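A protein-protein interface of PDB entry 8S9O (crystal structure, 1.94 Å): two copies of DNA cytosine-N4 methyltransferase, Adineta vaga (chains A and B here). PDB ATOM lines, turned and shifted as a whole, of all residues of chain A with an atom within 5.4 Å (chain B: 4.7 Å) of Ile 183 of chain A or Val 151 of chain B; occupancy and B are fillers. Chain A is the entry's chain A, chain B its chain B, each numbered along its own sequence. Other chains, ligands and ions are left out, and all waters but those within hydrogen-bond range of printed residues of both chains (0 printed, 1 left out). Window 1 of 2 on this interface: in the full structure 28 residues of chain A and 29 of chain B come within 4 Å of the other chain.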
ATOM      1  N   ILE A 133      12.303  -4.039 -20.094  1.00  0.00           N
ATOM      2  CA  ILE A 133      12.409  -5.491 -20.027  1.00  0.00           C
ATOM      3  C   ILE A 133      12.828  -5.863 -18.611  1.00  0.00           C
ATOM      4  O   ILE A 133      13.945  -5.559 -18.182  1.00  0.00           O
ATOM      5  CB  ILE A 133      13.402  -6.030 -21.065  1.00  0.00           C
ATOM      6  CG1 ILE A 133      13.011  -5.569 -22.471  1.00  0.00           C
ATOM      7  CG2 ILE A 133      13.472  -7.545 -20.999  1.00  0.00           C
ATOM      8  CD1 ILE A 133      11.627  -6.012 -22.900  1.00  0.00           C
ATOM      9  N   ASP A 135      14.014  -8.615 -16.384  1.00  0.00           N
ATOM     10  CA  ASP A 135      14.619  -9.941 -16.328  1.00  0.00           C
ATOM     11  C   ASP A 135      14.546 -10.424 -14.886  1.00  0.00           C
ATOM     12  O   ASP A 135      15.218  -9.879 -14.005  1.00  0.00           O
ATOM     13  CB  ASP A 135      16.059  -9.890 -16.833  1.00  0.00           C
ATOM     14  CG  ASP A 135      16.776 -11.231 -16.742  1.00  0.00           C
ATOM     15  OD1 ASP A 135      16.151 -12.251 -16.380  1.00  0.00           O
ATOM     16  OD2 ASP A 135      17.987 -11.260 -17.038  1.00  0.00           O
ATOM     17  N   TYR A 178      23.815  -0.180 -13.056  1.00  0.00           N
ATOM     18  CA  TYR A 178      23.137  -1.453 -13.271  1.00  0.00           C
ATOM     19  C   TYR A 178      21.728  -1.271 -13.825  1.00  0.00           C
ATOM     20  O   TYR A 178      21.228  -2.143 -14.545  1.00  0.00           O
ATOM     21  CB  TYR A 178      23.104  -2.214 -11.944  1.00  0.00           C
ATOM     22  CG  TYR A 178      22.841  -3.696 -12.038  1.00  0.00           C
ATOM     23  CD1 TYR A 178      23.810  -4.565 -12.525  1.00  0.00           C
ATOM     24  CD2 TYR A 178      21.639  -4.234 -11.601  1.00  0.00           C
ATOM     25  CE1 TYR A 178      23.576  -5.926 -12.596  1.00  0.00           C
ATOM     26  CE2 TYR A 178      21.397  -5.593 -11.667  1.00  0.00           C
ATOM     27  CZ  TYR A 178      22.368  -6.434 -12.165  1.00  0.00           C
ATOM     28  OH  TYR A 178      22.130  -7.786 -12.234  1.00  0.00           O
ATOM     29  N   PHE A 179      21.071  -0.152 -13.512  1.00  0.00           N
ATOM     30  CA  PHE A 179      19.672   0.049 -13.866  1.00  0.00           C
ATOM     31  C   PHE A 179      19.458   1.180 -14.865  1.00  0.00           C
ATOM     32  O   PHE A 179      18.320   1.632 -15.036  1.00  0.00           O
ATOM     33  CB  PHE A 179      18.847   0.303 -12.602  1.00  0.00           C
ATOM     34  CG  PHE A 179      18.705  -0.907 -11.725  1.00  0.00           C
ATOM     35  CD1 PHE A 179      18.321  -2.123 -12.262  1.00  0.00           C
ATOM     36  CD2 PHE A 179      18.970  -0.831 -10.369  1.00  0.00           C
ATOM     37  CE1 PHE A 179      18.190  -3.241 -11.460  1.00  0.00           C
ATOM     38  CE2 PHE A 179      18.843  -1.947  -9.562  1.00  0.00           C
ATOM     39  CZ  PHE A 179      18.453  -3.152 -10.107  1.00  0.00           C
ATOM     40  N   GLY A 181      19.971   0.832 -18.099  1.00  0.00           N
ATOM     41  CA  GLY A 181      19.608   0.235 -19.363  1.00  0.00           C
ATOM     42  C   GLY A 181      18.165  -0.249 -19.392  1.00  0.00           C
ATOM     43  O   GLY A 181      17.469  -0.296 -18.380  1.00  0.00           O
ATOM     44  N   VAL A 182      17.726  -0.626 -20.596  1.00  0.00           N
ATOM     45  CA  VAL A 182      16.332  -1.015 -20.808  1.00  0.00           C
ATOM     46  C   VAL A 182      16.017  -2.401 -20.264  1.00  0.00           C
ATOM     47  O   VAL A 182      14.842  -2.790 -20.232  1.00  0.00           O
ATOM     48  CB  VAL A 182      16.000  -0.900 -22.309  1.00  0.00           C
ATOM     49  CG1 VAL A 182      16.628  -2.041 -23.099  1.00  0.00           C
ATOM     50  CG2 VAL A 182      14.490  -0.814 -22.536  1.00  0.00           C
ATOM     51  N   ILE A 183      17.019  -3.155 -19.820  1.00  0.00           N
ATOM     52  CA  ILE A 183      16.806  -4.432 -19.145  1.00  0.00           C
ATOM     53  C   ILE A 183      17.152  -4.250 -17.674  1.00  0.00           C
ATOM     54  O   ILE A 183      18.267  -3.830 -17.340  1.00  0.00           O
ATOM     55  CB  ILE A 183      17.650  -5.562 -19.756  1.00  0.00           C
ATOM     56  CG1 ILE A 183      17.327  -5.758 -21.236  1.00  0.00           C
ATOM     57  CG2 ILE A 183      17.417  -6.865 -18.999  1.00  0.00           C
ATOM     58  CD1 ILE A 183      18.107  -6.905 -21.862  1.00  0.00           C
ATOM     59  N   TRP A 184      16.203  -4.570 -16.798  1.00  0.00           N
ATOM     60  CA  TRP A 184      16.427  -4.588 -15.358  1.00  0.00           C
ATOM     61  C   TRP A 184      16.480  -6.039 -14.900  1.00  0.00           C
ATOM     62  O   TRP A 184      15.509  -6.781 -15.074  1.00  0.00           O
ATOM     63  CB  TRP A 184      15.319  -3.853 -14.602  1.00  0.00           C
ATOM     64  CG  TRP A 184      15.065  -2.442 -15.022  1.00  0.00           C
ATOM     65  CD1 TRP A 184      15.855  -1.652 -15.805  1.00  0.00           C
ATOM     66  CD2 TRP A 184      13.925  -1.649 -14.670  1.00  0.00           C
ATOM     67  NE1 TRP A 184      15.273  -0.416 -15.967  1.00  0.00           N
ATOM     68  CE2 TRP A 184      14.089  -0.389 -15.278  1.00  0.00           C
ATOM     69  CE3 TRP A 184      12.783  -1.885 -13.900  1.00  0.00           C
ATOM     70  CZ2 TRP A 184      13.151   0.631 -15.140  1.00  0.00           C
ATOM     71  CZ3 TRP A 184      11.852  -0.871 -13.764  1.00  0.00           C
ATOM     72  CH2 TRP A 184      12.041   0.372 -14.383  1.00  0.00           C
ATOM     73  N   ARG A 185      17.604  -6.436 -14.310  1.00  0.00           N
ATOM     74  CA  ARG A 185      17.748  -7.770 -13.726  1.00  0.00           C
ATOM     75  C   ARG A 185      17.379  -7.674 -12.250  1.00  0.00           C
ATOM     76  O   ARG A 185      18.164  -7.191 -11.432  1.00  0.00           O
ATOM     77  CB  ARG A 185      19.165  -8.296 -13.920  1.00  0.00           C
ATOM     78  N   ILE B 133      14.091 -11.489 -26.954  1.00  0.00           N
ATOM     79  CA  ILE B 133      14.755 -10.230 -26.646  1.00  0.00           C
ATOM     80  C   ILE B 133      16.211 -10.359 -27.070  1.00  0.00           C
ATOM     81  O   ILE B 133      16.970 -11.143 -26.492  1.00  0.00           O
ATOM     82  CB  ILE B 133      14.640  -9.884 -25.156  1.00  0.00           C
ATOM     83  CG1 ILE B 133      13.173  -9.869 -24.720  1.00  0.00           C
ATOM     84  CG2 ILE B 133      15.312  -8.552 -24.864  1.00  0.00           C
ATOM     85  CD1 ILE B 133      12.329  -8.845 -25.445  1.00  0.00           C
ATOM     86  N   TRP B 134      16.608  -9.593 -28.081  1.00  0.00           N
ATOM     87  CA  TRP B 134      18.003  -9.529 -28.500  1.00  0.00           C
ATOM     88  C   TRP B 134      18.671  -8.388 -27.745  1.00  0.00           C
ATOM     89  O   TRP B 134      18.382  -7.214 -27.995  1.00  0.00           O
ATOM     90  CB  TRP B 134      18.115  -9.335 -30.012  1.00  0.00           C
ATOM     91  CG  TRP B 134      19.533  -9.158 -30.508  1.00  0.00           C
ATOM     92  CD1 TRP B 134      20.686  -9.443 -29.830  1.00  0.00           C
ATOM     93  CD2 TRP B 134      19.939  -8.647 -31.785  1.00  0.00           C
ATOM     94  NE1 TRP B 134      21.779  -9.138 -30.604  1.00  0.00           N
ATOM     95  CE2 TRP B 134      21.348  -8.650 -31.809  1.00  0.00           C
ATOM     96  CE3 TRP B 134      19.246  -8.187 -32.910  1.00  0.00           C
ATOM     97  CZ2 TRP B 134      22.076  -8.214 -32.913  1.00  0.00           C
ATOM     98  CZ3 TRP B 134      19.972  -7.753 -34.004  1.00  0.00           C
ATOM     99  CH2 TRP B 134      21.372  -7.771 -33.998  1.00  0.00           C
ATOM    100  N   ASP B 135      19.564  -8.735 -26.823  1.00  0.00           N
ATOM    101  CA  ASP B 135      20.369  -7.754 -26.106  1.00  0.00           C
ATOM    102  C   ASP B 135      21.670  -7.567 -26.876  1.00  0.00           C
ATOM    103  O   ASP B 135      22.510  -8.472 -26.919  1.00  0.00           O
ATOM    104  CB  ASP B 135      20.625  -8.219 -24.673  1.00  0.00           C
ATOM    105  CG  ASP B 135      21.489  -7.252 -23.877  1.00  0.00           C
ATOM    106  OD1 ASP B 135      21.859  -6.182 -24.406  1.00  0.00           O
ATOM    107  OD2 ASP B 135      21.802  -7.568 -22.710  1.00  0.00           O
ATOM    108  N   PRO B 149      18.648   2.120 -24.917  1.00  0.00           N
ATOM    109  CA  PRO B 149      17.913   1.222 -25.827  1.00  0.00           C
ATOM    110  C   PRO B 149      18.821   0.279 -26.616  1.00  0.00           C
ATOM    111  O   PRO B 149      19.066   0.429 -27.815  1.00  0.00           O
ATOM    112  CB  PRO B 149      17.190   2.207 -26.747  1.00  0.00           C
ATOM    113  CG  PRO B 149      18.150   3.358 -26.850  1.00  0.00           C
ATOM    114  CD  PRO B 149      18.876   3.445 -25.521  1.00  0.00           C
ATOM    115  N   TYR B 150      19.341  -0.735 -25.926  1.00  0.00           N
ATOM    116  CA  TYR B 150      20.230  -1.711 -26.543  1.00  0.00           C
ATOM    117  C   TYR B 150      19.534  -3.040 -26.818  1.00  0.00           C
ATOM    118  O   TYR B 150      20.200  -4.076 -26.910  1.00  0.00           O
ATOM    119  CB  TYR B 150      21.470  -1.928 -25.672  1.00  0.00           C
ATOM    120  CG  TYR B 150      21.182  -2.225 -24.215  1.00  0.00           C
ATOM    121  CD1 TYR B 150      20.614  -3.432 -23.829  1.00  0.00           C
ATOM    122  CD2 TYR B 150      21.499  -1.307 -23.225  1.00  0.00           C
ATOM    123  CE1 TYR B 150      20.355  -3.710 -22.502  1.00  0.00           C
ATOM    124  CE2 TYR B 150      21.245  -1.577 -21.892  1.00  0.00           C
ATOM    125  CZ  TYR B 150      20.673  -2.781 -21.537  1.00  0.00           C
ATOM    126  OH  TYR B 150      20.415  -3.061 -20.212  1.00  0.00           O
ATOM    127  N   VAL B 151      18.210  -3.032 -26.955  1.00  0.00           N
ATOM    128  CA  VAL B 151      17.423  -4.242 -27.155  1.00  0.00           C
ATOM    129  C   VAL B 151      16.640  -4.119 -28.455  1.00  0.00           C
ATOM    130  O   VAL B 151      16.056  -3.068 -28.742  1.00  0.00           O
ATOM    131  CB  VAL B 151      16.469  -4.501 -25.968  1.00  0.00           C
ATOM    132  CG1 VAL B 151      15.245  -5.297 -26.412  1.00  0.00           C
ATOM    133  CG2 VAL B 151      17.200  -5.229 -24.857  1.00  0.00           C
ATOM    134  N   GLU B 152      16.647  -5.189 -29.245  1.00  0.00           N
ATOM    135  CA  GLU B 152      15.748  -5.336 -30.377  1.00  0.00           C
ATOM    136  C   GLU B 152      14.919  -6.600 -30.195  1.00  0.00           C
ATOM    137  O   GLU B 152      15.353  -7.560 -29.552  1.00  0.00           O
ATOM    138  CB  GLU B 152      16.516  -5.385 -31.706  1.00  0.00           C
ATOM    139  CG  GLU B 152      17.264  -4.099 -32.016  1.00  0.00           C
ATOM    140  CD  GLU B 152      17.668  -3.987 -33.472  1.00  0.00           C
ATOM    141  OE1 GLU B 152      17.594  -5.003 -34.193  1.00  0.00           O
ATOM    142  OE2 GLU B 152      18.055  -2.877 -33.895  1.00  0.00           O
ATOM    143  N   LYS B 153      13.709  -6.582 -30.749  1.00  0.00           N
ATOM    144  CA  LYS B 153      12.796  -7.711 -30.655  1.00  0.00           C
ATOM    145  C   LYS B 153      12.989  -8.654 -31.834  1.00  0.00           C
ATOM    146  O   LYS B 153      13.202  -8.217 -32.969  1.00  0.00           O
ATOM    147  CB  LYS B 153      11.344  -7.234 -30.621  1.00  0.00           C
ATOM    148  CG  LYS B 153      10.940  -6.476 -29.369  1.00  0.00           C
ATOM    149  CD  LYS B 153       9.604  -5.785 -29.587  1.00  0.00           C
ATOM    150  CE  LYS B 153       9.060  -5.180 -28.307  1.00  0.00           C
ATOM    151  NZ  LYS B 153       7.791  -4.445 -28.568  1.00  0.00           N
ATOM    152  N   ILE B 183      16.271 -14.147 -23.499  1.00  0.00           N
ATOM    153  CA  ILE B 183      17.188 -13.044 -23.760  1.00  0.00           C
ATOM    154  C   ILE B 183      18.448 -13.621 -24.390  1.00  0.00           C
ATOM    155  O   ILE B 183      19.102 -14.491 -23.802  1.00  0.00           O
ATOM    156  CB  ILE B 183      17.532 -12.260 -22.483  1.00  0.00           C
ATOM    157  CG1 ILE B 183      16.274 -11.688 -21.832  1.00  0.00           C
ATOM    158  CG2 ILE B 183      18.512 -11.139 -22.803  1.00  0.00           C
ATOM    159  CD1 ILE B 183      16.570 -10.761 -20.665  1.00  0.00           C
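N of Ile 183 of chain A sits at hydrogen-bond distance from OH of Tyr 150 of chain B (3.4 Å).
Ile 133 of chain B touches its own counterpart, Ile 133 of chain A. Asp 135 of chain A touches Ile 183 of chain B, and with the chains exchanged Ile 183 of chain A touches Asp 135 of chain B. Positions printed for both chains: 133, 135 and 183. Of the 8 pairs that touch across the chains among the printed residues, 3 have their exchanged pair printed and touching as well.
The backbone NH (N) of Ile 133 of chain A sits at hydrogen-bond distance from the backbone carbonyl oxygen (O) of Val 182 of chain A (2.8 Å). N of Trp 184 of chain A is in hydrogen-bond range of O of Ile 133 of chain A (2.8 Å). N of Asp 135 of chain A sits at hydrogen-bond distance from O of Trp 184 of chain A (2.7 Å). The backbone carbonyl oxygen (O) of Gly 181 of chain A lies within hydrogen-bond range of the indole nitrogen (NE1) of Trp 184 of chain A, at 3.3 Å.
Printed residues of chain B within 4 Å of Ile 183 of chain A: Asp 135, Tyr 150 and Val 151. Of chain A, only Val 182 and Ile 183 come within 4 Å of Val 151 of chain B. Of the printed residues of chain B, Asp 135 of chain A touches Ile 183. Printed residues of chain A within 4 Å of Ile 133 of chain B: Ile 133. Printed residues of chain B within 4 Å of Ile 133 of chain A: Ile 133 (3.9 Å). Printed residues of chain A within 4 Å of Asp 135 of chain B: Ile 183. Of the printed residues of chain A, Tyr 150 of chain B touches Gly 181 (3.5 Å), Val 182 (3.6 Å) and Ile 183 (3.4 Å). Glu 152 of chain B touches none of the printed residues of chain A. The nearest residue of chain B that does not touch Ile 183 of chain A is Ile 183 of chain B (4.3 Å). The nearest printed residue of chain A that does not touch Ile 133 of chain B is Ile 183 of chain A (4.4 Å).
Ile 133 of chain A touches Ile 133 of chain B (CD1 to CD1, 3.9 Å). Asp 135 of chain A touches Ile 183 of chain B. Gly 181 of chain A touches Tyr 150 of chain B. OH of Tyr 150 of chain B touches N of Val 182 of chain A, at 3.6 Å. CG1 of Val 182 of chain A touches CG2 of Val 151 of chain B, 3.7 Å away. Ile 183 of chain A touches Asp 135 of chain B. CG2 of Val 151 of chain B touches CD1 of Ile 183 of chain A, at 3.5 Å.
Of the 9 printed residues of chain B, 5 touch a printed residue of chain A. Hydrophobic or aromatic side chains of chain B within 4 Å of the printed part of chain A: Ile 133, Tyr 150, Val 151 and Ile 183. Among the printed residues, no Asp or Glu carboxylate lies within 4 Å of a Lys or Arg side-chain nitrogen of the other chain.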
